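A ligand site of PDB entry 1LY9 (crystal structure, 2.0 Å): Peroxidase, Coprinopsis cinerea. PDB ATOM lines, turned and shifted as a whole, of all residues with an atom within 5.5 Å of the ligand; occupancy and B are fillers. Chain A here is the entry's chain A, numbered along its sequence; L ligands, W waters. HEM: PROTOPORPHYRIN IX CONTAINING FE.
A ring nitrogen (NE2) of His 183 binds an iron atom (FE) of the ligand. O2D of the ligand lies within hydrogen-bond range of N of Ser 187 (3.1 Å). The backbone NH (N) of Gly 190 lies within hydrogen-bond range of an oxygen (O1A) of the ligand, 2.8 Å away. An oxygen (O2D) of the ligand lies within hydrogen-bond range of the side-chain hydroxyl (OG) of Ser 187, at 2.7 Å. An oxygen (O2A) of the ligand sits at hydrogen-bond distance from the backbone NH (N) of Glu 189 (3.1 Å). The guanidinium group of Arg 51 is in salt-bridge range of an oxygen (O2A) of the ligand (3.9 Å). The guanidinium group (NE) of Arg 47 is in salt-bridge range of an oxygen (O2D) of the ligand, at 2.7 Å.
SD of Met 242 lies within hydrogen-bond range of OG of Ser 244, 3.5 Å away. SD of Met 276 lies close to OH of Tyr 272, at 3.7 Å. N of Leu 191 sits at hydrogen-bond distance from OE1 of Gln 188. The backbone NH of Leu 200 is in hydrogen-bond range of the backbone carbonyl oxygen of Ala 186, at 2.9 Å. The side-chain carboxylate (OE1) of Glu 189 is in salt-bridge range of the side-chain amino group (NZ) of Lys 48 (2.7 Å).
Lys 48 touches the ligand. O of Leu 50 touches CAC of the ligand (3.5 Å). CE1 of Phe 54 touches CHC of the ligand, 3.5 Å away. O of Pro 153 touches CMB of the ligand, at 3.8 Å. C of Gly 154 touches CMB of the ligand (3.3 Å). N of Pro 155 touches CMB of the ligand, at 3.5 Å. Leu 179 touches the ligand (CB to CMC, 3.7 Å). Leu 180 touches the ligand (CD2 to CHC, 3.5 Å). Ala 182 touches the ligand (CB to CBC, 3.5 Å). O of Leu 185 touches CMD of the ligand (3.3 Å). Ala 186 touches the ligand. CA of Gln 188 touches O2A of the ligand (3.8 Å). Leu 191 touches the ligand (N to O1A, 3.6 Å). Met 242 touches the ligand (SD to CHB, 3.5 Å). Ser 244 touches the ligand. OH of Tyr 272 touches CBC of the ligand, 3.7 Å away. Met 276 touches the ligand. Hydrophobic or aromatic side chains within 4 Å of the ligand: Leu 50, Phe 54, Pro 155, Leu 179, Leu 180, Ala 182, His 183, Ala 186, Leu 191, Met 242, Tyr 272 and Met 276.
Water W4 lies within hydrogen-bond range of an oxygen (O1D) of the ligand (2.6 Å), the side-chain carboxylate of Glu 189 (2.8 Å), the guanidinium group of Arg 47 (3.0 Å) and the side-chain hydroxyl of Ser 44 (3.0 Å). Water W2 lies within hydrogen-bond range of an oxygen (O2A) of the ligand (2.6 Å), the side-chain amino group of Lys 48 (2.7 Å) and the guanidinium group of Arg 51 (2.8 Å).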
ATOM      1  N   SER A  44     -19.653  16.809  10.707  1.00  0.00           N
ATOM      2  CA  SER A  44     -19.230  15.723  11.603  1.00  0.00           C
ATOM      3  C   SER A  44     -19.100  16.085  13.081  1.00  0.00           C
ATOM      4  O   SER A  44     -19.565  15.340  13.937  1.00  0.00           O
ATOM      5  CB  SER A  44     -17.912  15.115  11.112  1.00  0.00           C
ATOM      6  OG  SER A  44     -17.558  13.995  11.904  1.00  0.00           O
ATOM      7  N   VAL A  46     -20.693  18.058  14.907  1.00  0.00           N
ATOM      8  CA  VAL A  46     -21.997  18.116  15.558  1.00  0.00           C
ATOM      9  C   VAL A  46     -22.493  16.696  15.818  1.00  0.00           C
ATOM     10  O   VAL A  46     -22.988  16.390  16.903  1.00  0.00           O
ATOM     11  CB  VAL A  46     -23.043  18.845  14.672  1.00  0.00           C
ATOM     12  CG1 VAL A  46     -24.450  18.725  15.290  1.00  0.00           C
ATOM     13  CG2 VAL A  46     -22.667  20.300  14.517  1.00  0.00           C
ATOM     14  N   ARG A  47     -22.342  15.842  14.817  1.00  0.00           N
ATOM     15  CA  ARG A  47     -22.777  14.448  14.911  1.00  0.00           C
ATOM     16  C   ARG A  47     -22.017  13.675  15.985  1.00  0.00           C
ATOM     17  O   ARG A  47     -22.616  12.874  16.715  1.00  0.00           O
ATOM     18  CB  ARG A  47     -22.642  13.767  13.539  1.00  0.00           C
ATOM     19  CG  ARG A  47     -23.407  14.483  12.425  1.00  0.00           C
ATOM     20  CD  ARG A  47     -23.632  13.585  11.215  1.00  0.00           C
ATOM     21  NE  ARG A  47     -22.380  13.125  10.610  1.00  0.00           N
ATOM     22  CZ  ARG A  47     -21.693  13.800   9.697  1.00  0.00           C
ATOM     23  NH1 ARG A  47     -22.131  14.982   9.268  1.00  0.00           N
ATOM     24  NH2 ARG A  47     -20.578  13.296   9.196  1.00  0.00           N
ATOM     25  N   LYS A  48     -20.720  13.920  16.090  1.00  0.00           N
ATOM     26  CA  LYS A  48     -19.871  13.264  17.088  1.00  0.00           C
ATOM     27  C   LYS A  48     -20.232  13.725  18.500  1.00  0.00           C
ATOM     28  O   LYS A  48     -20.218  12.932  19.437  1.00  0.00           O
ATOM     29  CB  LYS A  48     -18.400  13.580  16.829  1.00  0.00           C
ATOM     30  CG  LYS A  48     -17.851  13.019  15.533  1.00  0.00           C
ATOM     31  CD  LYS A  48     -17.684  11.512  15.609  1.00  0.00           C
ATOM     32  CE  LYS A  48     -16.982  10.981  14.363  1.00  0.00           C
ATOM     33  NZ  LYS A  48     -16.811   9.506  14.405  1.00  0.00           N
ATOM     34  N   LEU A  50     -23.118  14.702  19.521  1.00  0.00           N
ATOM     35  CA  LEU A  50     -24.400  14.085  19.878  1.00  0.00           C
ATOM     36  C   LEU A  50     -24.188  12.651  20.366  1.00  0.00           C
ATOM     37  O   LEU A  50     -24.920  12.176  21.229  1.00  0.00           O
ATOM     38  CB  LEU A  50     -25.366  14.122  18.695  1.00  0.00           C
ATOM     39  CG  LEU A  50     -26.074  15.469  18.462  1.00  0.00           C
ATOM     40  CD1 LEU A  50     -26.733  15.488  17.092  1.00  0.00           C
ATOM     41  CD2 LEU A  50     -27.119  15.676  19.556  1.00  0.00           C
ATOM     42  N   ARG A  51     -23.188  11.961  19.815  1.00  0.00           N
ATOM     43  CA  ARG A  51     -22.912  10.602  20.286  1.00  0.00           C
ATOM     44  C   ARG A  51     -22.308  10.718  21.687  1.00  0.00           C
ATOM     45  O   ARG A  51     -22.662   9.957  22.589  1.00  0.00           O
ATOM     46  CB  ARG A  51     -21.911   9.881  19.371  1.00  0.00           C
ATOM     47  CG  ARG A  51     -22.507   9.259  18.116  1.00  0.00           C
ATOM     48  CD  ARG A  51     -21.439   8.480  17.329  1.00  0.00           C
ATOM     49  NE  ARG A  51     -20.903   7.334  18.072  1.00  0.00           N
ATOM     50  CZ  ARG A  51     -19.669   6.860  17.919  1.00  0.00           C
ATOM     51  NH1 ARG A  51     -18.838   7.425  17.053  1.00  0.00           N
ATOM     52  NH2 ARG A  51     -19.267   5.821  18.631  1.00  0.00           N
ATOM     53  N   VAL A  53     -22.664  13.142  24.022  1.00  0.00           N
ATOM     54  CA  VAL A  53     -23.593  13.521  25.079  1.00  0.00           C
ATOM     55  C   VAL A  53     -24.430  12.314  25.529  1.00  0.00           C
ATOM     56  O   VAL A  53     -24.638  12.129  26.735  1.00  0.00           O
ATOM     57  CB  VAL A  53     -24.526  14.686  24.641  1.00  0.00           C
ATOM     58  CG1 VAL A  53     -25.507  14.243  23.551  1.00  0.00           C
ATOM     59  CG2 VAL A  53     -25.279  15.235  25.862  1.00  0.00           C
ATOM     60  N   PHE A  54     -24.867  11.499  24.575  1.00  0.00           N
ATOM     61  CA  PHE A  54     -25.655  10.297  24.899  1.00  0.00           C
ATOM     62  C   PHE A  54     -24.822   9.296  25.701  1.00  0.00           C
ATOM     63  O   PHE A  54     -25.267   8.787  26.735  1.00  0.00           O
ATOM     64  CB  PHE A  54     -26.139   9.626  23.602  1.00  0.00           C
ATOM     65  CG  PHE A  54     -26.847   8.302  23.821  1.00  0.00           C
ATOM     66  CD1 PHE A  54     -26.673   7.257  22.908  1.00  0.00           C
ATOM     67  CD2 PHE A  54     -27.712   8.108  24.895  1.00  0.00           C
ATOM     68  CE1 PHE A  54     -27.349   6.045  23.076  1.00  0.00           C
ATOM     69  CE2 PHE A  54     -28.396   6.897  25.068  1.00  0.00           C
ATOM     70  CZ  PHE A  54     -28.212   5.871  24.152  1.00  0.00           C
ATOM     71  N   PRO A 153     -26.284   1.172  25.161  1.00  0.00           N
ATOM     72  CA  PRO A 153     -27.029   0.296  24.251  1.00  0.00           C
ATOM     73  C   PRO A 153     -26.328   0.259  22.889  1.00  0.00           C
ATOM     74  O   PRO A 153     -25.826   1.281  22.433  1.00  0.00           O
ATOM     75  CB  PRO A 153     -28.397   0.976  24.162  1.00  0.00           C
ATOM     76  CG  PRO A 153     -28.517   1.681  25.480  1.00  0.00           C
ATOM     77  CD  PRO A 153     -27.128   2.263  25.660  1.00  0.00           C
ATOM     78  N   GLY A 154     -26.307  -0.903  22.248  1.00  0.00           N
ATOM     79  CA  GLY A 154     -25.664  -1.009  20.948  1.00  0.00           C
ATOM     80  C   GLY A 154     -26.584  -1.540  19.866  1.00  0.00           C
ATOM     81  O   GLY A 154     -27.651  -2.075  20.181  1.00  0.00           O
ATOM     82  N   PRO A 155     -26.200  -1.408  18.588  1.00  0.00           N
ATOM     83  CA  PRO A 155     -27.020  -1.886  17.473  1.00  0.00           C
ATOM     84  C   PRO A 155     -27.159  -3.400  17.408  1.00  0.00           C
ATOM     85  O   PRO A 155     -27.966  -3.928  16.650  1.00  0.00           O
ATOM     86  CB  PRO A 155     -26.286  -1.303  16.254  1.00  0.00           C
ATOM     87  CG  PRO A 155     -24.871  -1.379  16.678  1.00  0.00           C
ATOM     88  CD  PRO A 155     -24.908  -0.873  18.105  1.00  0.00           C
ATOM     89  N   ILE A 162     -32.489  -3.039  24.876  1.00  0.00           N
ATOM     90  CA  ILE A 162     -32.350  -1.592  24.763  1.00  0.00           C
ATOM     91  C   ILE A 162     -33.380  -0.884  25.634  1.00  0.00           C
ATOM     92  O   ILE A 162     -33.061   0.074  26.339  1.00  0.00           O
ATOM     93  CB  ILE A 162     -32.491  -1.156  23.291  1.00  0.00           C
ATOM     94  CG1 ILE A 162     -31.319  -1.732  22.480  1.00  0.00           C
ATOM     95  CG2 ILE A 162     -32.510   0.368  23.184  1.00  0.00           C
ATOM     96  CD1 ILE A 162     -31.358  -1.387  20.990  1.00  0.00           C
ATOM     97  N   MET A 166     -32.410   1.465  28.881  1.00  0.00           N
ATOM     98  CA  MET A 166     -32.897   2.839  28.894  1.00  0.00           C
ATOM     99  C   MET A 166     -33.917   3.051  30.008  1.00  0.00           C
ATOM    100  O   MET A 166     -33.968   4.129  30.609  1.00  0.00           O
ATOM    101  CB  MET A 166     -33.525   3.196  27.543  1.00  0.00           C
ATOM    102  CG  MET A 166     -32.543   3.215  26.368  1.00  0.00           C
ATOM    103  SD  MET A 166     -31.263   4.485  26.541  1.00  0.00           S
ATOM    104  CE  MET A 166     -32.090   5.932  25.838  1.00  0.00           C
ATOM    105  N   VAL A 176     -37.462   6.813  24.354  1.00  0.00           N
ATOM    106  CA  VAL A 176     -36.333   6.233  23.642  1.00  0.00           C
ATOM    107  C   VAL A 176     -36.507   6.572  22.165  1.00  0.00           C
ATOM    108  O   VAL A 176     -35.545   6.897  21.467  1.00  0.00           O
ATOM    109  CB  VAL A 176     -36.277   4.690  23.807  1.00  0.00           C
ATOM    110  CG1 VAL A 176     -35.271   4.084  22.835  1.00  0.00           C
ATOM    111  CG2 VAL A 176     -35.893   4.332  25.242  1.00  0.00           C
ATOM    112  N   LEU A 179     -35.701  10.359  21.664  1.00  0.00           N
ATOM    113  CA  LEU A 179     -34.264  10.636  21.685  1.00  0.00           C
ATOM    114  C   LEU A 179     -33.582  10.253  20.378  1.00  0.00           C
ATOM    115  O   LEU A 179     -32.588  10.874  19.979  1.00  0.00           O
ATOM    116  CB  LEU A 179     -33.585   9.885  22.837  1.00  0.00           C
ATOM    117  CG  LEU A 179     -33.770  10.418  24.254  1.00  0.00           C
ATOM    118  CD1 LEU A 179     -33.188   9.418  25.240  1.00  0.00           C
ATOM    119  CD2 LEU A 179     -33.085  11.775  24.402  1.00  0.00           C
ATOM    120  N   LEU A 180     -34.102   9.222  19.719  1.00  0.00           N
ATOM    121  CA  LEU A 180     -33.526   8.757  18.457  1.00  0.00           C
ATOM    122  C   LEU A 180     -33.689   9.744  17.309  1.00  0.00           C
ATOM    123  O   LEU A 180     -33.151   9.520  16.226  1.00  0.00           O
ATOM    124  CB  LEU A 180     -34.133   7.389  18.079  1.00  0.00           C
ATOM    125  CG  LEU A 180     -33.442   6.201  18.752  1.00  0.00           C
ATOM    126  CD1 LEU A 180     -34.235   4.921  18.542  1.00  0.00           C
ATOM    127  CD2 LEU A 180     -32.033   6.065  18.178  1.00  0.00           C
ATOM    128  N   ALA A 182     -32.236  12.179  16.947  1.00  0.00           N
ATOM    129  CA  ALA A 182     -30.881  12.630  16.662  1.00  0.00           C
ATOM    130  C   ALA A 182     -30.291  11.844  15.486  1.00  0.00           C
ATOM    131  O   ALA A 182     -29.271  12.254  14.907  1.00  0.00           O
ATOM    132  CB  ALA A 182     -29.997  12.477  17.892  1.00  0.00           C
ATOM    133  N   HIS A 183     -30.898  10.716  15.143  1.00  0.00           N
ATOM    134  CA  HIS A 183     -30.414   9.936  14.024  1.00  0.00           C
ATOM    135  C   HIS A 183     -30.853  10.602  12.718  1.00  0.00           C
ATOM    136  O   HIS A 183     -30.646  10.051  11.630  1.00  0.00           O
ATOM    137  CB  HIS A 183     -30.934   8.494  14.082  1.00  0.00           C
ATOM    138  CG  HIS A 183     -30.079   7.580  14.894  1.00  0.00           C
ATOM    139  ND1 HIS A 183     -30.124   6.209  14.814  1.00  0.00           N
ATOM    140  CD2 HIS A 183     -29.119   7.856  15.818  1.00  0.00           C
ATOM    141  CE1 HIS A 183     -29.219   5.700  15.667  1.00  0.00           C
ATOM    142  NE2 HIS A 183     -28.582   6.671  16.290  1.00  0.00           N
ATOM    143  N   LEU A 185     -29.657  13.406  12.000  1.00  0.00           N
ATOM    144  CA  LEU A 185     -28.403  14.132  11.702  1.00  0.00           C
ATOM    145  C   LEU A 185     -27.316  13.098  11.941  1.00  0.00           C
ATOM    146  O   LEU A 185     -26.429  13.288  12.779  1.00  0.00           O
ATOM    147  CB  LEU A 185     -28.200  15.282  12.688  1.00  0.00           C
ATOM    148  CG  LEU A 185     -29.187  16.444  12.739  1.00  0.00           C
ATOM    149  CD1 LEU A 185     -28.790  17.401  13.860  1.00  0.00           C
ATOM    150  CD2 LEU A 185     -29.207  17.168  11.412  1.00  0.00           C
ATOM    151  N   ALA A 186     -27.376  12.002  11.207  1.00  0.00           N
ATOM    152  CA  ALA A 186     -26.433  10.923  11.448  1.00  0.00           C
ATOM    153  C   ALA A 186     -25.904  10.144  10.252  1.00  0.00           C
ATOM    154  O   ALA A 186     -26.507  10.124   9.175  1.00  0.00           O
ATOM    155  CB  ALA A 186     -27.056   9.953  12.431  1.00  0.00           C
ATOM    156  N   SER A 187     -24.772   9.490  10.472  1.00  0.00           N
ATOM    157  CA  SER A 187     -24.135   8.642   9.484  1.00  0.00           C
ATOM    158  C   SER A 187     -23.427   7.610  10.337  1.00  0.00           C
ATOM    159  O   SER A 187     -23.483   7.689  11.569  1.00  0.00           O
ATOM    160  CB  SER A 187     -23.110   9.435   8.660  1.00  0.00           C
ATOM    161  OG  SER A 187     -21.881   9.579   9.367  1.00  0.00           O
ATOM    162  N   GLN A 188     -22.800   6.635   9.695  1.00  0.00           N
ATOM    163  CA  GLN A 188     -22.031   5.626  10.417  1.00  0.00           C
ATOM    164  C   GLN A 188     -20.649   5.588   9.792  1.00  0.00           C
ATOM    165  O   GLN A 188     -20.504   5.790   8.581  1.00  0.00           O
ATOM    166  CB  GLN A 188     -22.694   4.243  10.324  1.00  0.00           C
ATOM    167  CG  GLN A 188     -22.818   3.642   8.914  1.00  0.00           C
ATOM    168  CD  GLN A 188     -21.535   2.969   8.412  1.00  0.00           C
ATOM    169  OE1 GLN A 188     -20.768   2.409   9.202  1.00  0.00           O
ATOM    170  NE2 GLN A 188     -21.332   2.991   7.102  1.00  0.00           N
ATOM    171  N   GLU A 189     -19.638   5.333  10.602  1.00  0.00           N
ATOM    172  CA  GLU A 189     -18.271   5.254  10.124  1.00  0.00           C
ATOM    173  C   GLU A 189     -17.684   3.885  10.430  1.00  0.00           C
ATOM    174  O   GLU A 189     -16.867   3.363   9.674  1.00  0.00           O
ATOM    175  CB  GLU A 189     -17.398   6.349  10.769  1.00  0.00           C
ATOM    176  CG  GLU A 189     -17.904   7.772  10.564  1.00  0.00           C
ATOM    177  CD  GLU A 189     -16.925   8.827  11.064  1.00  0.00           C
ATOM    178  OE1 GLU A 189     -16.108   8.516  11.966  1.00  0.00           O
ATOM    179  OE2 GLU A 189     -16.967   9.971  10.568  1.00  0.00           O
ATOM    180  N   GLY A 190     -18.132   3.281  11.523  1.00  0.00           N
ATOM    181  CA  GLY A 190     -17.586   1.982  11.889  1.00  0.00           C
ATOM    182  C   GLY A 190     -18.434   0.732  11.755  1.00  0.00           C
ATOM    183  O   GLY A 190     -17.944  -0.371  12.019  1.00  0.00           O
ATOM    184  N   LEU A 191     -19.693   0.860  11.347  1.00  0.00           N
ATOM    185  CA  LEU A 191     -20.533  -0.329  11.204  1.00  0.00           C
ATOM    186  C   LEU A 191     -20.274  -1.048   9.879  1.00  0.00           C
ATOM    187  O   LEU A 191     -20.419  -2.266   9.778  1.00  0.00           O
ATOM    188  CB  LEU A 191     -22.006   0.042  11.327  1.00  0.00           C
ATOM    189  CG  LEU A 191     -22.416   0.581  12.710  1.00  0.00           C
ATOM    190  CD1 LEU A 191     -23.908   0.893  12.718  1.00  0.00           C
ATOM    191  CD2 LEU A 191     -22.076  -0.450  13.786  1.00  0.00           C
ATOM    192  N   LEU A 200     -27.993   8.173   7.693  1.00  0.00           N
ATOM    193  CA  LEU A 200     -29.076   7.359   8.228  1.00  0.00           C
ATOM    194  C   LEU A 200     -30.415   7.804   7.631  1.00  0.00           C
ATOM    195  O   LEU A 200     -31.396   7.050   7.655  1.00  0.00           O
ATOM    196  CB  LEU A 200     -29.095   7.431   9.758  1.00  0.00           C
ATOM    197  CG  LEU A 200     -28.405   6.259  10.482  1.00  0.00           C
ATOM    198  CD1 LEU A 200     -27.175   5.792   9.734  1.00  0.00           C
ATOM    199  CD2 LEU A 200     -28.051   6.673  11.896  1.00  0.00           C
ATOM    200  N   MET A 242     -29.447   0.790  10.250  1.00  0.00           N
ATOM    201  CA  MET A 242     -28.966   0.088  11.440  1.00  0.00           C
ATOM    202  C   MET A 242     -30.041  -0.886  11.946  1.00  0.00           C
ATOM    203  O   MET A 242     -31.220  -0.539  11.974  1.00  0.00           O
ATOM    204  CB  MET A 242     -28.654   1.130  12.496  1.00  0.00           C
ATOM    205  CG  MET A 242     -27.902   0.659  13.716  1.00  0.00           C
ATOM    206  SD  MET A 242     -27.604   2.062  14.811  1.00  0.00           S
ATOM    207  CE  MET A 242     -26.865   3.234  13.676  1.00  0.00           C
ATOM    208  N   SER A 244     -30.905  -1.952  14.959  1.00  0.00           N
ATOM    209  CA  SER A 244     -31.697  -1.462  16.088  1.00  0.00           C
ATOM    210  C   SER A 244     -32.764  -0.466  15.662  1.00  0.00           C
ATOM    211  O   SER A 244     -33.886  -0.495  16.160  1.00  0.00           O
ATOM    212  CB  SER A 244     -30.779  -0.850  17.159  1.00  0.00           C
ATOM    213  OG  SER A 244     -29.839   0.052  16.598  1.00  0.00           O
ATOM    214  N   LEU A 248     -36.724  -1.136  16.144  1.00  0.00           N
ATOM    215  CA  LEU A 248     -37.482  -0.214  16.993  1.00  0.00           C
ATOM    216  C   LEU A 248     -38.666   0.407  16.251  1.00  0.00           C
ATOM    217  O   LEU A 248     -39.721   0.675  16.846  1.00  0.00           O
ATOM    218  CB  LEU A 248     -36.571   0.886  17.531  1.00  0.00           C
ATOM    219  CG  LEU A 248     -35.619   0.451  18.652  1.00  0.00           C
ATOM    220  CD1 LEU A 248     -34.669   1.573  18.990  1.00  0.00           C
ATOM    221  CD2 LEU A 248     -36.432   0.067  19.880  1.00  0.00           C
ATOM    222  N   TYR A 272     -38.177  15.734  21.260  1.00  0.00           N
ATOM    223  CA  TYR A 272     -36.747  15.499  21.388  1.00  0.00           C
ATOM    224  C   TYR A 272     -36.166  16.443  22.425  1.00  0.00           C
ATOM    225  O   TYR A 272     -35.366  16.016  23.274  1.00  0.00           O
ATOM    226  CB  TYR A 272     -36.078  15.727  20.026  1.00  0.00           C
ATOM    227  CG  TYR A 272     -34.567  15.693  20.060  1.00  0.00           C
ATOM    228  CD1 TYR A 272     -33.825  16.873  20.073  1.00  0.00           C
ATOM    229  CD2 TYR A 272     -33.876  14.480  20.036  1.00  0.00           C
ATOM    230  CE1 TYR A 272     -32.432  16.855  20.053  1.00  0.00           C
ATOM    231  CE2 TYR A 272     -32.485  14.442  20.014  1.00  0.00           C
ATOM    232  CZ  TYR A 272     -31.769  15.636  20.021  1.00  0.00           C
ATOM    233  OH  TYR A 272     -30.401  15.605  19.944  1.00  0.00           O
ATOM    234  N   MET A 276     -34.280  15.348  25.746  1.00  0.00           N
ATOM    235  CA  MET A 276     -32.891  15.756  25.959  1.00  0.00           C
ATOM    236  C   MET A 276     -32.719  16.457  27.306  1.00  0.00           C
ATOM    237  O   MET A 276     -31.726  16.233  28.013  1.00  0.00           O
ATOM    238  CB  MET A 276     -32.425  16.684  24.831  1.00  0.00           C
ATOM    239  CG  MET A 276     -32.201  16.000  23.486  1.00  0.00           C
ATOM    240  SD  MET A 276     -30.843  14.792  23.514  1.00  0.00           S
ATOM    241  CE  MET A 276     -29.410  15.834  23.316  1.00  0.00           C
ATOM    242  N   MET A 279     -32.368  13.872  29.878  1.00  0.00           N
ATOM    243  CA  MET A 279     -31.075  13.191  29.835  1.00  0.00           C
ATOM    244  C   MET A 279     -29.949  14.054  30.393  1.00  0.00           C
ATOM    245  O   MET A 279     -28.997  13.541  30.987  1.00  0.00           O
ATOM    246  CB  MET A 279     -30.741  12.766  28.398  1.00  0.00           C
ATOM    247  CG  MET A 279     -29.535  11.838  28.278  1.00  0.00           C
ATOM    248  SD  MET A 279     -29.298  11.159  26.602  1.00  0.00           S
ATOM    249  CE  MET A 279     -28.491  12.538  25.814  1.00  0.00           C
HETATM  250  CHA HEM L   1     -24.702   7.050  15.398  1.00  0.00           C
HETATM  251  CHB HEM L   1     -26.349   3.333  17.799  1.00  0.00           C
HETATM  252  CHC HEM L   1     -29.063   6.486  20.003  1.00  0.00           C
HETATM  253  CHD HEM L   1     -26.795  10.119  18.198  1.00  0.00           C
HETATM  254  C1A HEM L   1     -24.778   5.804  15.811  1.00  0.00           C
HETATM  255  C2A HEM L   1     -23.971   4.610  15.393  1.00  0.00           C
HETATM  256  C3A HEM L   1     -24.336   3.551  16.138  1.00  0.00           C
HETATM  257  C4A HEM L   1     -25.512   4.092  17.018  1.00  0.00           C
HETATM  258  CMA HEM L   1     -23.743   2.063  16.279  1.00  0.00           C
HETATM  259  CAA HEM L   1     -22.879   4.574  14.247  1.00  0.00           C
HETATM  260  CBA HEM L   1     -21.526   5.058  14.949  1.00  0.00           C
HETATM  261  CGA HEM L   1     -20.373   4.992  13.844  1.00  0.00           C
HETATM  262  O1A HEM L   1     -20.203   3.827  13.287  1.00  0.00           O
HETATM  263  O2A HEM L   1     -19.885   6.081  13.563  1.00  0.00           O
HETATM  264  C1B HEM L   1     -27.420   3.758  18.594  1.00  0.00           C
HETATM  265  C2B HEM L   1     -28.313   2.981  19.420  1.00  0.00           C
HETATM  266  C3B HEM L   1     -29.192   3.908  20.119  1.00  0.00           C
HETATM  267  C4B HEM L   1     -28.688   5.203  19.643  1.00  0.00           C
HETATM  268  CMB HEM L   1     -28.275   1.292  19.551  1.00  0.00           C
HETATM  269  CAB HEM L   1     -30.388   3.367  21.174  1.00  0.00           C
HETATM  270  CBB HEM L   1     -31.258   4.306  22.217  1.00  0.00           C
HETATM  271  C1C HEM L   1     -28.638   7.783  19.865  1.00  0.00           C
HETATM  272  C2C HEM L   1     -29.050   8.924  20.788  1.00  0.00           C
HETATM  273  C3C HEM L   1     -28.358  10.025  20.343  1.00  0.00           C
HETATM  274  C4C HEM L   1     -27.530   9.397  19.134  1.00  0.00           C
HETATM  275  CMC HEM L   1     -30.074   8.815  22.144  1.00  0.00           C
HETATM  276  CAC HEM L   1     -28.301  11.423  20.825  1.00  0.00           C
HETATM  277  CBC HEM L   1     -29.354  12.343  21.348  1.00  0.00           C
HETATM  278  C1D HEM L   1     -26.126   9.655  17.043  1.00  0.00           C
HETATM  279  C2D HEM L   1     -25.531  10.465  15.958  1.00  0.00           C
HETATM  280  C3D HEM L   1     -24.886   9.567  15.209  1.00  0.00           C
HETATM  281  C4D HEM L   1     -25.127   8.281  15.721  1.00  0.00           C
HETATM  282  CMD HEM L   1     -25.717  12.113  15.785  1.00  0.00           C
HETATM  283  CAD HEM L   1     -23.974   9.961  13.967  1.00  0.00           C
HETATM  284  CBD HEM L   1     -22.538  10.084  14.276  1.00  0.00           C
HETATM  285  CGD HEM L   1     -21.665  10.437  12.850  1.00  0.00           C
HETATM  286  O1D HEM L   1     -20.562  10.499  13.111  1.00  0.00           O
HETATM  287  O2D HEM L   1     -22.196  10.699  11.805  1.00  0.00           O
HETATM  288  NA  HEM L   1     -25.600   5.461  16.800  1.00  0.00           N
HETATM  289  NB  HEM L   1     -27.644   5.176  18.697  1.00  0.00           N
HETATM  290  NC  HEM L   1     -27.780   8.083  18.990  1.00  0.00           N
HETATM  291  ND  HEM L   1     -25.950   8.330  16.841  1.00  0.00           N
HETATM  292 FE   HEM L   1     -26.761   6.829  17.781  1.00  0.00          FE
HETATM  293  O   HOH W   1     -24.959   6.422  19.679  1.00  0.00           O
HETATM  294  O   HOH W   2     -19.293   8.467  14.473  1.00  0.00           O
HETATM  295  O   HOH W   3     -30.927   2.493  17.322  1.00  0.00           O
HETATM  296  O   HOH W   4     -19.163  11.553  11.166  1.00  0.00           O
HETATM  297  O   HOH W   5     -19.325   1.859  15.016  1.00  0.00           O
HETATM  298  O   HOH W   6     -24.735   3.048  20.815  1.00  0.00           O
HETATM  299  O   HOH W   7     -16.868   5.395  14.415  1.00  0.00           O
